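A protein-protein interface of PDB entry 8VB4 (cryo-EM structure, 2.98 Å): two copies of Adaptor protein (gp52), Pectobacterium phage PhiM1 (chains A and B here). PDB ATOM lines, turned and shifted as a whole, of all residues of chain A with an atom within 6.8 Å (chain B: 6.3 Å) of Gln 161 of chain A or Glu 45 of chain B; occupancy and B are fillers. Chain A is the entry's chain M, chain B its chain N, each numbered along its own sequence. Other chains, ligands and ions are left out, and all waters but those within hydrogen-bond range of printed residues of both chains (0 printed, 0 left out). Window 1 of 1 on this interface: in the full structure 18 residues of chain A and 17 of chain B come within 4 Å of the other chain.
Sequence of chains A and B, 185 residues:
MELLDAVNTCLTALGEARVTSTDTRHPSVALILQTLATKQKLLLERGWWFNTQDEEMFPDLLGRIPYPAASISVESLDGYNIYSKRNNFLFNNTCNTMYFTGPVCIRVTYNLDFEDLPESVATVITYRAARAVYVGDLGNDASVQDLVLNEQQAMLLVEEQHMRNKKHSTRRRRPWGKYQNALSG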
ATOM      1  N   TRP A  49      11.672 -34.695  21.930  1.00  0.00           N
ATOM      2  CA  TRP A  49      10.352 -34.891  22.513  1.00  0.00           C
ATOM      3  C   TRP A  49       9.309 -35.353  21.503  1.00  0.00           C
ATOM      4  O   TRP A  49       8.180 -35.651  21.907  1.00  0.00           O
ATOM      5  CB  TRP A  49       9.874 -33.595  23.175  1.00  0.00           C
ATOM      6  CG  TRP A  49       9.229 -32.618  22.231  1.00  0.00           C
ATOM      7  CD1 TRP A  49       7.894 -32.479  21.983  1.00  0.00           C
ATOM      8  CD2 TRP A  49       9.890 -31.638  21.419  1.00  0.00           C
ATOM      9  NE1 TRP A  49       7.685 -31.479  21.065  1.00  0.00           N
ATOM     10  CE2 TRP A  49       8.894 -30.947  20.704  1.00  0.00           C
ATOM     11  CE3 TRP A  49      11.228 -31.282  21.227  1.00  0.00           C
ATOM     12  CZ2 TRP A  49       9.193 -29.922  19.812  1.00  0.00           C
ATOM     13  CZ3 TRP A  49      11.522 -30.263  20.340  1.00  0.00           C
ATOM     14  CH2 TRP A  49      10.509 -29.595  19.645  1.00  0.00           C
ATOM     15  N   PRO A 118       9.561 -29.572  13.090  1.00  0.00           N
ATOM     16  CA  PRO A 118       9.242 -28.186  13.441  1.00  0.00           C
ATOM     17  C   PRO A 118      10.124 -27.199  12.688  1.00  0.00           C
ATOM     18  O   PRO A 118      11.163 -27.550  12.127  1.00  0.00           O
ATOM     19  CB  PRO A 118       9.505 -28.129  14.951  1.00  0.00           C
ATOM     20  CG  PRO A 118       9.357 -29.530  15.412  1.00  0.00           C
ATOM     21  CD  PRO A 118       9.851 -30.385  14.285  1.00  0.00           C
ATOM     22  N   GLU A 119       9.684 -25.938  12.681  1.00  0.00           N
ATOM     23  CA  GLU A 119      10.410 -24.900  11.957  1.00  0.00           C
ATOM     24  C   GLU A 119      11.820 -24.725  12.508  1.00  0.00           C
ATOM     25  O   GLU A 119      12.783 -24.567  11.749  1.00  0.00           O
ATOM     26  CB  GLU A 119       9.640 -23.581  12.030  1.00  0.00           C
ATOM     27  CG  GLU A 119       8.322 -23.589  11.278  1.00  0.00           C
ATOM     28  CD  GLU A 119       8.511 -23.631   9.774  1.00  0.00           C
ATOM     29  OE1 GLU A 119       9.503 -23.057   9.283  1.00  0.00           O
ATOM     30  OE2 GLU A 119       7.666 -24.240   9.084  1.00  0.00           O
ATOM     31  N   SER A 120      11.957 -24.739  13.834  1.00  0.00           N
ATOM     32  CA  SER A 120      13.258 -24.491  14.446  1.00  0.00           C
ATOM     33  C   SER A 120      14.269 -25.566  14.060  1.00  0.00           C
ATOM     34  O   SER A 120      15.435 -25.262  13.786  1.00  0.00           O
ATOM     35  CB  SER A 120      13.105 -24.408  15.963  1.00  0.00           C
ATOM     36  OG  SER A 120      12.621 -25.630  16.494  1.00  0.00           O
ATOM     37  N   LEU A 156      19.278 -22.434  20.118  1.00  0.00           N
ATOM     38  CA  LEU A 156      18.757 -21.976  21.403  1.00  0.00           C
ATOM     39  C   LEU A 156      17.241 -22.131  21.476  1.00  0.00           C
ATOM     40  O   LEU A 156      16.712 -22.640  22.475  1.00  0.00           O
ATOM     41  CB  LEU A 156      19.150 -20.519  21.648  1.00  0.00           C
ATOM     42  CG  LEU A 156      20.621 -20.262  21.981  1.00  0.00           C
ATOM     43  CD1 LEU A 156      20.899 -18.771  22.028  1.00  0.00           C
ATOM     44  CD2 LEU A 156      21.003 -20.919  23.297  1.00  0.00           C
ATOM     45  N   LEU A 157      16.528 -21.709  20.429  1.00  0.00           N
ATOM     46  CA  LEU A 157      15.077 -21.866  20.407  1.00  0.00           C
ATOM     47  C   LEU A 157      14.680 -23.336  20.420  1.00  0.00           C
ATOM     48  O   LEU A 157      13.703 -23.713  21.076  1.00  0.00           O
ATOM     49  CB  LEU A 157      14.494 -21.168  19.179  1.00  0.00           C
ATOM     50  CG  LEU A 157      14.643 -19.648  19.124  1.00  0.00           C
ATOM     51  CD1 LEU A 157      14.184 -19.121  17.775  1.00  0.00           C
ATOM     52  CD2 LEU A 157      13.865 -18.986  20.248  1.00  0.00           C
ATOM     53  N   VAL A 158      15.414 -24.178  19.689  1.00  0.00           N
ATOM     54  CA  VAL A 158      15.105 -25.606  19.683  1.00  0.00           C
ATOM     55  C   VAL A 158      15.180 -26.166  21.096  1.00  0.00           C
ATOM     56  O   VAL A 158      14.276 -26.882  21.553  1.00  0.00           O
ATOM     57  CB  VAL A 158      16.058 -26.358  18.735  1.00  0.00           C
ATOM     58  CG1 VAL A 158      15.981 -27.858  18.978  1.00  0.00           C
ATOM     59  CG2 VAL A 158      15.742 -26.035  17.288  1.00  0.00           C
ATOM     60  N   GLU A 159      16.263 -25.854  21.810  1.00  0.00           N
ATOM     61  CA  GLU A 159      16.430 -26.375  23.162  1.00  0.00           C
ATOM     62  C   GLU A 159      15.354 -25.836  24.095  1.00  0.00           C
ATOM     63  O   GLU A 159      14.825 -26.575  24.935  1.00  0.00           O
ATOM     64  CB  GLU A 159      17.823 -26.026  23.687  1.00  0.00           C
ATOM     65  CG  GLU A 159      18.154 -26.607  25.059  1.00  0.00           C
ATOM     66  CD  GLU A 159      17.668 -28.033  25.243  1.00  0.00           C
ATOM     67  OE1 GLU A 159      17.269 -28.386  26.374  1.00  0.00           O
ATOM     68  OE2 GLU A 159      17.702 -28.809  24.265  1.00  0.00           O
ATOM     69  N   GLU A 160      15.021 -24.550  23.972  1.00  0.00           N
ATOM     70  CA  GLU A 160      13.975 -23.981  24.816  1.00  0.00           C
ATOM     71  C   GLU A 160      12.645 -24.686  24.581  1.00  0.00           C
ATOM     72  O   GLU A 160      11.927 -25.021  25.530  1.00  0.00           O
ATOM     73  CB  GLU A 160      13.850 -22.479  24.549  1.00  0.00           C
ATOM     74  CG  GLU A 160      12.733 -21.785  25.319  1.00  0.00           C
ATOM     75  CD  GLU A 160      12.442 -20.395  24.791  1.00  0.00           C
ATOM     76  OE1 GLU A 160      11.299 -20.151  24.353  1.00  0.00           O
ATOM     77  OE2 GLU A 160      13.356 -19.545  24.817  1.00  0.00           O
ATOM     78  N   GLN A 161      12.301 -24.924  23.313  1.00  0.00           N
ATOM     79  CA  GLN A 161      11.049 -25.601  22.995  1.00  0.00           C
ATOM     80  C   GLN A 161      11.031 -27.017  23.558  1.00  0.00           C
ATOM     81  O   GLN A 161      10.031 -27.446  24.151  1.00  0.00           O
ATOM     82  CB  GLN A 161      10.845 -25.618  21.480  1.00  0.00           C
ATOM     83  CG  GLN A 161       9.536 -26.232  21.015  1.00  0.00           C
ATOM     84  CD  GLN A 161       8.323 -25.473  21.517  1.00  0.00           C
ATOM     85  OE1 GLN A 161       8.001 -24.395  21.019  1.00  0.00           O
ATOM     86  NE2 GLN A 161       7.641 -26.037  22.508  1.00  0.00           N
ATOM     87  N   HIS A 162      12.131 -27.756  23.390  1.00  0.00           N
ATOM     88  CA  HIS A 162      12.176 -29.117  23.918  1.00  0.00           C
ATOM     89  C   HIS A 162      12.022 -29.122  25.432  1.00  0.00           C
ATOM     90  O   HIS A 162      11.295 -29.956  25.985  1.00  0.00           O
ATOM     91  CB  HIS A 162      13.480 -29.805  23.521  1.00  0.00           C
ATOM     92  CG  HIS A 162      13.728 -31.086  24.256  1.00  0.00           C
ATOM     93  ND1 HIS A 162      13.210 -32.294  23.843  1.00  0.00           N
ATOM     94  CD2 HIS A 162      14.431 -31.345  25.384  1.00  0.00           C
ATOM     95  CE1 HIS A 162      13.588 -33.243  24.682  1.00  0.00           C
ATOM     96  NE2 HIS A 162      14.329 -32.693  25.626  1.00  0.00           N
ATOM     97  N   MET A 163      12.701 -28.204  26.122  1.00  0.00           N
ATOM     98  CA  MET A 163      12.563 -28.135  27.573  1.00  0.00           C
ATOM     99  C   MET A 163      11.131 -27.798  27.970  1.00  0.00           C
ATOM    100  O   MET A 163      10.617 -28.322  28.964  1.00  0.00           O
ATOM    101  CB  MET A 163      13.532 -27.102  28.143  1.00  0.00           C
ATOM    102  CG  MET A 163      13.794 -27.259  29.630  1.00  0.00           C
ATOM    103  SD  MET A 163      14.976 -28.568  29.990  1.00  0.00           S
ATOM    104  CE  MET A 163      14.674 -28.817  31.736  1.00  0.00           C
ATOM    105  N   ARG A 164      10.476 -26.919  27.210  1.00  0.00           N
ATOM    106  CA  ARG A 164       9.100 -26.550  27.531  1.00  0.00           C
ATOM    107  C   ARG A 164       8.150 -27.732  27.370  1.00  0.00           C
ATOM    108  O   ARG A 164       7.260 -27.934  28.204  1.00  0.00           O
ATOM    109  CB  ARG A 164       8.653 -25.384  26.650  1.00  0.00           C
ATOM    110  CG  ARG A 164       7.196 -24.996  26.841  1.00  0.00           C
ATOM    111  CD  ARG A 164       6.820 -23.751  26.052  1.00  0.00           C
ATOM    112  NE  ARG A 164       7.735 -22.639  26.284  1.00  0.00           N
ATOM    113  CZ  ARG A 164       7.916 -21.627  25.447  1.00  0.00           C
ATOM    114  NH1 ARG A 164       7.254 -21.548  24.304  1.00  0.00           N
ATOM    115  NH2 ARG A 164       8.776 -20.666  25.767  1.00  0.00           N
ATOM    116  N   ASN A 165       8.313 -28.521  26.304  1.00  0.00           N
ATOM    117  CA  ASN A 165       7.346 -29.582  26.026  1.00  0.00           C
ATOM    118  C   ASN A 165       7.444 -30.726  27.031  1.00  0.00           C
ATOM    119  O   ASN A 165       6.425 -31.320  27.400  1.00  0.00           O
ATOM    120  CB  ASN A 165       7.534 -30.109  24.606  1.00  0.00           C
ATOM    121  CG  ASN A 165       7.257 -29.059  23.553  1.00  0.00           C
ATOM    122  OD1 ASN A 165       8.155 -28.644  22.821  1.00  0.00           O
ATOM    123  ND2 ASN A 165       6.006 -28.626  23.466  1.00  0.00           N
ATOM    124  N   LYS A 166       8.657 -31.060  27.478  1.00  0.00           N
ATOM    125  CA  LYS A 166       8.833 -32.255  28.302  1.00  0.00           C
ATOM    126  C   LYS A 166       8.139 -32.116  29.653  1.00  0.00           C
ATOM    127  O   LYS A 166       7.615 -33.098  30.189  1.00  0.00           O
ATOM    128  CB  LYS A 166      10.320 -32.547  28.493  1.00  0.00           C
ATOM    129  CG  LYS A 166      11.001 -33.135  27.263  1.00  0.00           C
ATOM    130  CD  LYS A 166      10.554 -34.565  26.980  1.00  0.00           C
ATOM    131  CE  LYS A 166      11.088 -35.542  28.013  1.00  0.00           C
ATOM    132  NZ  LYS A 166      10.822 -36.954  27.627  1.00  0.00           N
ATOM    133  N   GLN B  40       9.183 -13.839   8.832  1.00  0.00           N
ATOM    134  CA  GLN B  40       7.963 -13.652   9.609  1.00  0.00           C
ATOM    135  C   GLN B  40       7.491 -14.970  10.204  1.00  0.00           C
ATOM    136  O   GLN B  40       7.096 -15.027  11.374  1.00  0.00           O
ATOM    137  CB  GLN B  40       6.871 -13.045   8.733  1.00  0.00           C
ATOM    138  CG  GLN B  40       5.546 -12.833   9.447  1.00  0.00           C
ATOM    139  CD  GLN B  40       4.471 -12.297   8.527  1.00  0.00           C
ATOM    140  OE1 GLN B  40       4.703 -12.089   7.337  1.00  0.00           O
ATOM    141  NE2 GLN B  40       3.282 -12.075   9.074  1.00  0.00           N
ATOM    142  N   LYS B  41       7.518 -16.044   9.411  1.00  0.00           N
ATOM    143  CA  LYS B  41       7.085 -17.339   9.923  1.00  0.00           C
ATOM    144  C   LYS B  41       7.987 -17.811  11.055  1.00  0.00           C
ATOM    145  O   LYS B  41       7.504 -18.350  12.059  1.00  0.00           O
ATOM    146  CB  LYS B  41       7.061 -18.370   8.795  1.00  0.00           C
ATOM    147  CG  LYS B  41       6.789 -19.790   9.269  1.00  0.00           C
ATOM    148  CD  LYS B  41       6.263 -20.672   8.149  1.00  0.00           C
ATOM    149  CE  LYS B  41       5.375 -21.782   8.688  1.00  0.00           C
ATOM    150  NZ  LYS B  41       4.854 -22.660   7.606  1.00  0.00           N
ATOM    151  N   LEU B  42       9.300 -17.621  10.915  1.00  0.00           N
ATOM    152  CA  LEU B  42      10.217 -18.085  11.952  1.00  0.00           C
ATOM    153  C   LEU B  42      10.060 -17.285  13.241  1.00  0.00           C
ATOM    154  O   LEU B  42      10.085 -17.857  14.336  1.00  0.00           O
ATOM    155  CB  LEU B  42      11.659 -18.010  11.451  1.00  0.00           C
ATOM    156  CG  LEU B  42      12.752 -18.303  12.483  1.00  0.00           C
ATOM    157  CD1 LEU B  42      12.645 -19.727  13.004  1.00  0.00           C
ATOM    158  CD2 LEU B  42      14.126 -18.056  11.880  1.00  0.00           C
ATOM    159  N   LEU B  43       9.901 -15.962  13.135  1.00  0.00           N
ATOM    160  CA  LEU B  43       9.922 -15.123  14.331  1.00  0.00           C
ATOM    161  C   LEU B  43       8.769 -15.448  15.272  1.00  0.00           C
ATOM    162  O   LEU B  43       8.958 -15.530  16.490  1.00  0.00           O
ATOM    163  CB  LEU B  43       9.884 -13.647  13.934  1.00  0.00           C
ATOM    164  CG  LEU B  43       9.734 -12.642  15.081  1.00  0.00           C
ATOM    165  CD1 LEU B  43      10.817 -12.844  16.128  1.00  0.00           C
ATOM    166  CD2 LEU B  43       9.763 -11.219  14.552  1.00  0.00           C
ATOM    167  N   LEU B  44       7.568 -15.640  14.729  1.00  0.00           N
ATOM    168  CA  LEU B  44       6.368 -15.777  15.546  1.00  0.00           C
ATOM    169  C   LEU B  44       6.178 -17.182  16.106  1.00  0.00           C
ATOM    170  O   LEU B  44       5.150 -17.441  16.740  1.00  0.00           O
ATOM    171  CB  LEU B  44       5.134 -15.390  14.725  1.00  0.00           C
ATOM    172  CG  LEU B  44       5.139 -13.980  14.127  1.00  0.00           C
ATOM    173  CD1 LEU B  44       3.871 -13.740  13.325  1.00  0.00           C
ATOM    174  CD2 LEU B  44       5.292 -12.925  15.210  1.00  0.00           C
ATOM    175  N   GLU B  45       7.133 -18.089  15.893  1.00  0.00           N
ATOM    176  CA  GLU B  45       6.950 -19.472  16.321  1.00  0.00           C
ATOM    177  C   GLU B  45       6.819 -19.578  17.837  1.00  0.00           C
ATOM    178  O   GLU B  45       5.984 -20.337  18.343  1.00  0.00           O
ATOM    179  CB  GLU B  45       8.114 -20.324  15.822  1.00  0.00           C
ATOM    180  CG  GLU B  45       7.916 -21.822  16.004  1.00  0.00           C
ATOM    181  CD  GLU B  45       8.496 -22.342  17.306  1.00  0.00           C
ATOM    182  OE1 GLU B  45       9.027 -21.533  18.094  1.00  0.00           O
ATOM    183  OE2 GLU B  45       8.422 -23.568  17.540  1.00  0.00           O
ATOM    184  N   ARG B  46       7.636 -18.827  18.580  1.00  0.00           N
ATOM    185  CA  ARG B  46       7.642 -18.966  20.034  1.00  0.00           C
ATOM    186  C   ARG B  46       6.304 -18.556  20.641  1.00  0.00           C
ATOM    187  O   ARG B  46       5.823 -19.195  21.585  1.00  0.00           O
ATOM    188  CB  ARG B  46       8.789 -18.146  20.633  1.00  0.00           C
ATOM    189  CG  ARG B  46       8.471 -16.679  20.894  1.00  0.00           C
ATOM    190  CD  ARG B  46       9.648 -15.963  21.533  1.00  0.00           C
ATOM    191  NE  ARG B  46       9.946 -16.480  22.862  1.00  0.00           N
ATOM    192  CZ  ARG B  46      11.102 -16.312  23.491  1.00  0.00           C
ATOM    193  NH1 ARG B  46      12.097 -15.634  22.942  1.00  0.00           N
ATOM    194  NH2 ARG B  46      11.263 -16.836  24.703  1.00  0.00           N
ATOM    195  N   GLY B  47       5.694 -17.493  20.122  1.00  0.00           N
ATOM    196  CA  GLY B  47       4.434 -17.007  20.652  1.00  0.00           C
ATOM    197  C   GLY B  47       4.581 -15.702  21.407  1.00  0.00           C
ATOM    198  O   GLY B  47       5.546 -15.515  22.151  1.00  0.00           O
ATOM    199  N   TRP B  48       3.625 -14.795  21.228  1.00  0.00           N
ATOM    200  CA  TRP B  48       3.667 -13.475  21.845  1.00  0.00           C
ATOM    201  C   TRP B  48       2.290 -13.174  22.428  1.00  0.00           C
ATOM    202  O   TRP B  48       1.431 -14.055  22.531  1.00  0.00           O
ATOM    203  CB  TRP B  48       4.118 -12.418  20.828  1.00  0.00           C
ATOM    204  CG  TRP B  48       5.487 -12.667  20.285  1.00  0.00           C
ATOM    205  CD1 TRP B  48       5.808 -13.368  19.160  1.00  0.00           C
ATOM    206  CD2 TRP B  48       6.727 -12.218  20.844  1.00  0.00           C
ATOM    207  NE1 TRP B  48       7.170 -13.383  18.984  1.00  0.00           N
ATOM    208  CE2 TRP B  48       7.757 -12.683  20.005  1.00  0.00           C
ATOM    209  CE3 TRP B  48       7.065 -11.466  21.973  1.00  0.00           C
ATOM    210  CZ2 TRP B  48       9.100 -12.422  20.259  1.00  0.00           C
ATOM    211  CZ3 TRP B  48       8.399 -11.208  22.222  1.00  0.00           C
ATOM    212  CH2 TRP B  48       9.399 -11.685  21.370  1.00  0.00           C
ATOM    213  N   ASN B  51      -0.808 -13.385  19.486  1.00  0.00           N
ATOM    214  CA  ASN B  51      -1.059 -14.523  18.610  1.00  0.00           C
ATOM    215  C   ASN B  51      -1.072 -15.839  19.381  1.00  0.00           C
ATOM    216  O   ASN B  51      -0.614 -16.867  18.869  1.00  0.00           O
ATOM    217  CB  ASN B  51      -0.019 -14.580  17.487  1.00  0.00           C
ATOM    218  CG  ASN B  51       1.347 -15.018  17.977  1.00  0.00           C
ATOM    219  OD1 ASN B  51       1.769 -14.661  19.075  1.00  0.00           O
ATOM    220  ND2 ASN B  51       2.048 -15.791  17.157  1.00  0.00           N
ATOM    221  N   ILE B  72       1.265 -22.705  13.882  1.00  0.00           N
ATOM    222  CA  ILE B  72       2.681 -22.979  13.680  1.00  0.00           C
ATOM    223  C   ILE B  72       3.224 -24.005  14.668  1.00  0.00           C
ATOM    224  O   ILE B  72       4.173 -24.726  14.323  1.00  0.00           O
ATOM    225  CB  ILE B  72       3.516 -21.683  13.757  1.00  0.00           C
ATOM    226  CG1 ILE B  72       3.102 -20.718  12.643  1.00  0.00           C
ATOM    227  CG2 ILE B  72       5.004 -22.005  13.666  1.00  0.00           C
ATOM    228  CD1 ILE B  72       3.792 -19.370  12.706  1.00  0.00           C
ATOM    229  N   SER B  73       2.665 -24.099  15.874  1.00  0.00           N
ATOM    230  CA  SER B  73       3.148 -25.040  16.873  1.00  0.00           C
ATOM    231  C   SER B  73       1.980 -25.492  17.736  1.00  0.00           C
ATOM    232  O   SER B  73       0.998 -24.762  17.895  1.00  0.00           O
ATOM    233  CB  SER B  73       4.238 -24.416  17.748  1.00  0.00           C
ATOM    234  OG  SER B  73       3.719 -23.358  18.534  1.00  0.00           O
ATOM    235  N   VAL B  74       2.093 -26.698  18.286  1.00  0.00           N
ATOM    236  CA  VAL B  74       1.058 -27.285  19.127  1.00  0.00           C
ATOM    237  C   VAL B  74       1.686 -27.746  20.433  1.00  0.00           C
ATOM    238  O   VAL B  74       2.854 -28.146  20.479  1.00  0.00           O
ATOM    239  CB  VAL B  74       0.344 -28.460  18.424  1.00  0.00           C
ATOM    240  CG1 VAL B  74      -0.726 -29.050  19.332  1.00  0.00           C
ATOM    241  CG2 VAL B  74      -0.252 -28.003  17.097  1.00  0.00           C
ATOM    242  N   GLU B  75       0.896 -27.688  21.503  1.00  0.00           N
ATOM    243  CA  GLU B  75       1.331 -28.138  22.816  1.00  0.00           C
ATOM    244  C   GLU B  75       0.125 -28.672  23.570  1.00  0.00           C
ATOM    245  O   GLU B  75      -1.018 -28.313  23.272  1.00  0.00           O
ATOM    246  CB  GLU B  75       2.001 -27.008  23.606  1.00  0.00           C
ATOM    247  CG  GLU B  75       2.637 -27.454  24.911  1.00  0.00           C
ATOM    248  CD  GLU B  75       3.370 -26.333  25.614  1.00  0.00           C
ATOM    249  OE1 GLU B  75       3.275 -26.247  26.856  1.00  0.00           O
ATOM    250  OE2 GLU B  75       4.042 -25.536  24.926  1.00  0.00           O
ATOM    251  N   THR B 109      -0.332 -21.462  18.242  1.00  0.00           N
ATOM    252  CA  THR B 109       0.305 -20.220  17.823  1.00  0.00           C
ATOM    253  C   THR B 109      -0.045 -19.976  16.361  1.00  0.00           C
ATOM    254  O   THR B 109       0.235 -20.822  15.506  1.00  0.00           O
ATOM    255  CB  THR B 109       1.820 -20.288  18.012  1.00  0.00           C
ATOM    256  OG1 THR B 109       2.120 -20.818  19.309  1.00  0.00           O
ATOM    257  CG2 THR B 109       2.441 -18.908  17.880  1.00  0.00           C
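OE2 of Glu 119 of chain A lies within salt-bridge range of NZ of Lys 41 of chain B (3.5 Å). The side-chain carboxylate of Glu 160 of chain A is in salt-bridge range of the guanidinium group of Arg 46 of chain B, 3.3 Å away.
NE1 of Trp 49 of chain A lies close to OD1 of Asn 165 of chain A (3.4 Å). OE1 of Glu 160 of chain A is in salt-bridge range of NH2 of Arg 164 of chain A (2.9 Å). The backbone carbonyl oxygen (O) of Gln 161 of chain A lies close to the side-chain amide oxygen (OD1) of Asn 165 of chain A, 2.6 Å away.
Among the printed residues, merely in contact across the chains: Arg 164 of chain A with Glu 75 of chain B (3.5 Å), Gln 161 of chain A with Glu 45 of chain B (3.6 Å), Asn 165 of chain A with Glu 75 of chain B (3.8 Å) and Arg 164 of chain A with Arg 46 of chain B (3.9 Å).
Of the printed residues of chain B, Glu 119 of chain A touches Lys 41. Of the printed residues of chain B, Glu 160 of chain A touches Arg 46. Of chain B, only Glu 45 comes within 4 Å of Gln 161 of chain A. Printed residues of chain B within 4 Å of Arg 164 of chain A: Arg 46 and Glu 75. Of the printed residues of chain A, Lys 41 of chain B touches Glu 119 (3.4 Å). Leu 42 of chain B touches none of the printed residues of chain A. Of chain A, only Gln 161 (3.6 Å) comes within 4 Å of Glu 45 of chain B. Of the printed residues of chain A, Glu 75 of chain B touches Arg 164 and Asn 165. The nearest residue of chain A that does not touch Glu 45 of chain B is Glu 119 of chain A (4.7 Å).
Of the 15 printed residues of chain B, 4 touch a printed residue of chain A. Among the printed residues, 6 pairs touch across the chains. Among the printed residues, Asp or Glu carboxylates within 4 Å of a Lys or Arg side-chain nitrogen of the other chain: Glu 119 of chain A with Lys 41 of chain B and Glu 160 of chain A with Arg 46 of chain B.
No position is printed for both chains. Of the 6 pairs that touch across the chains among the printed residues, none has its exchanged pair printed and touching as well.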
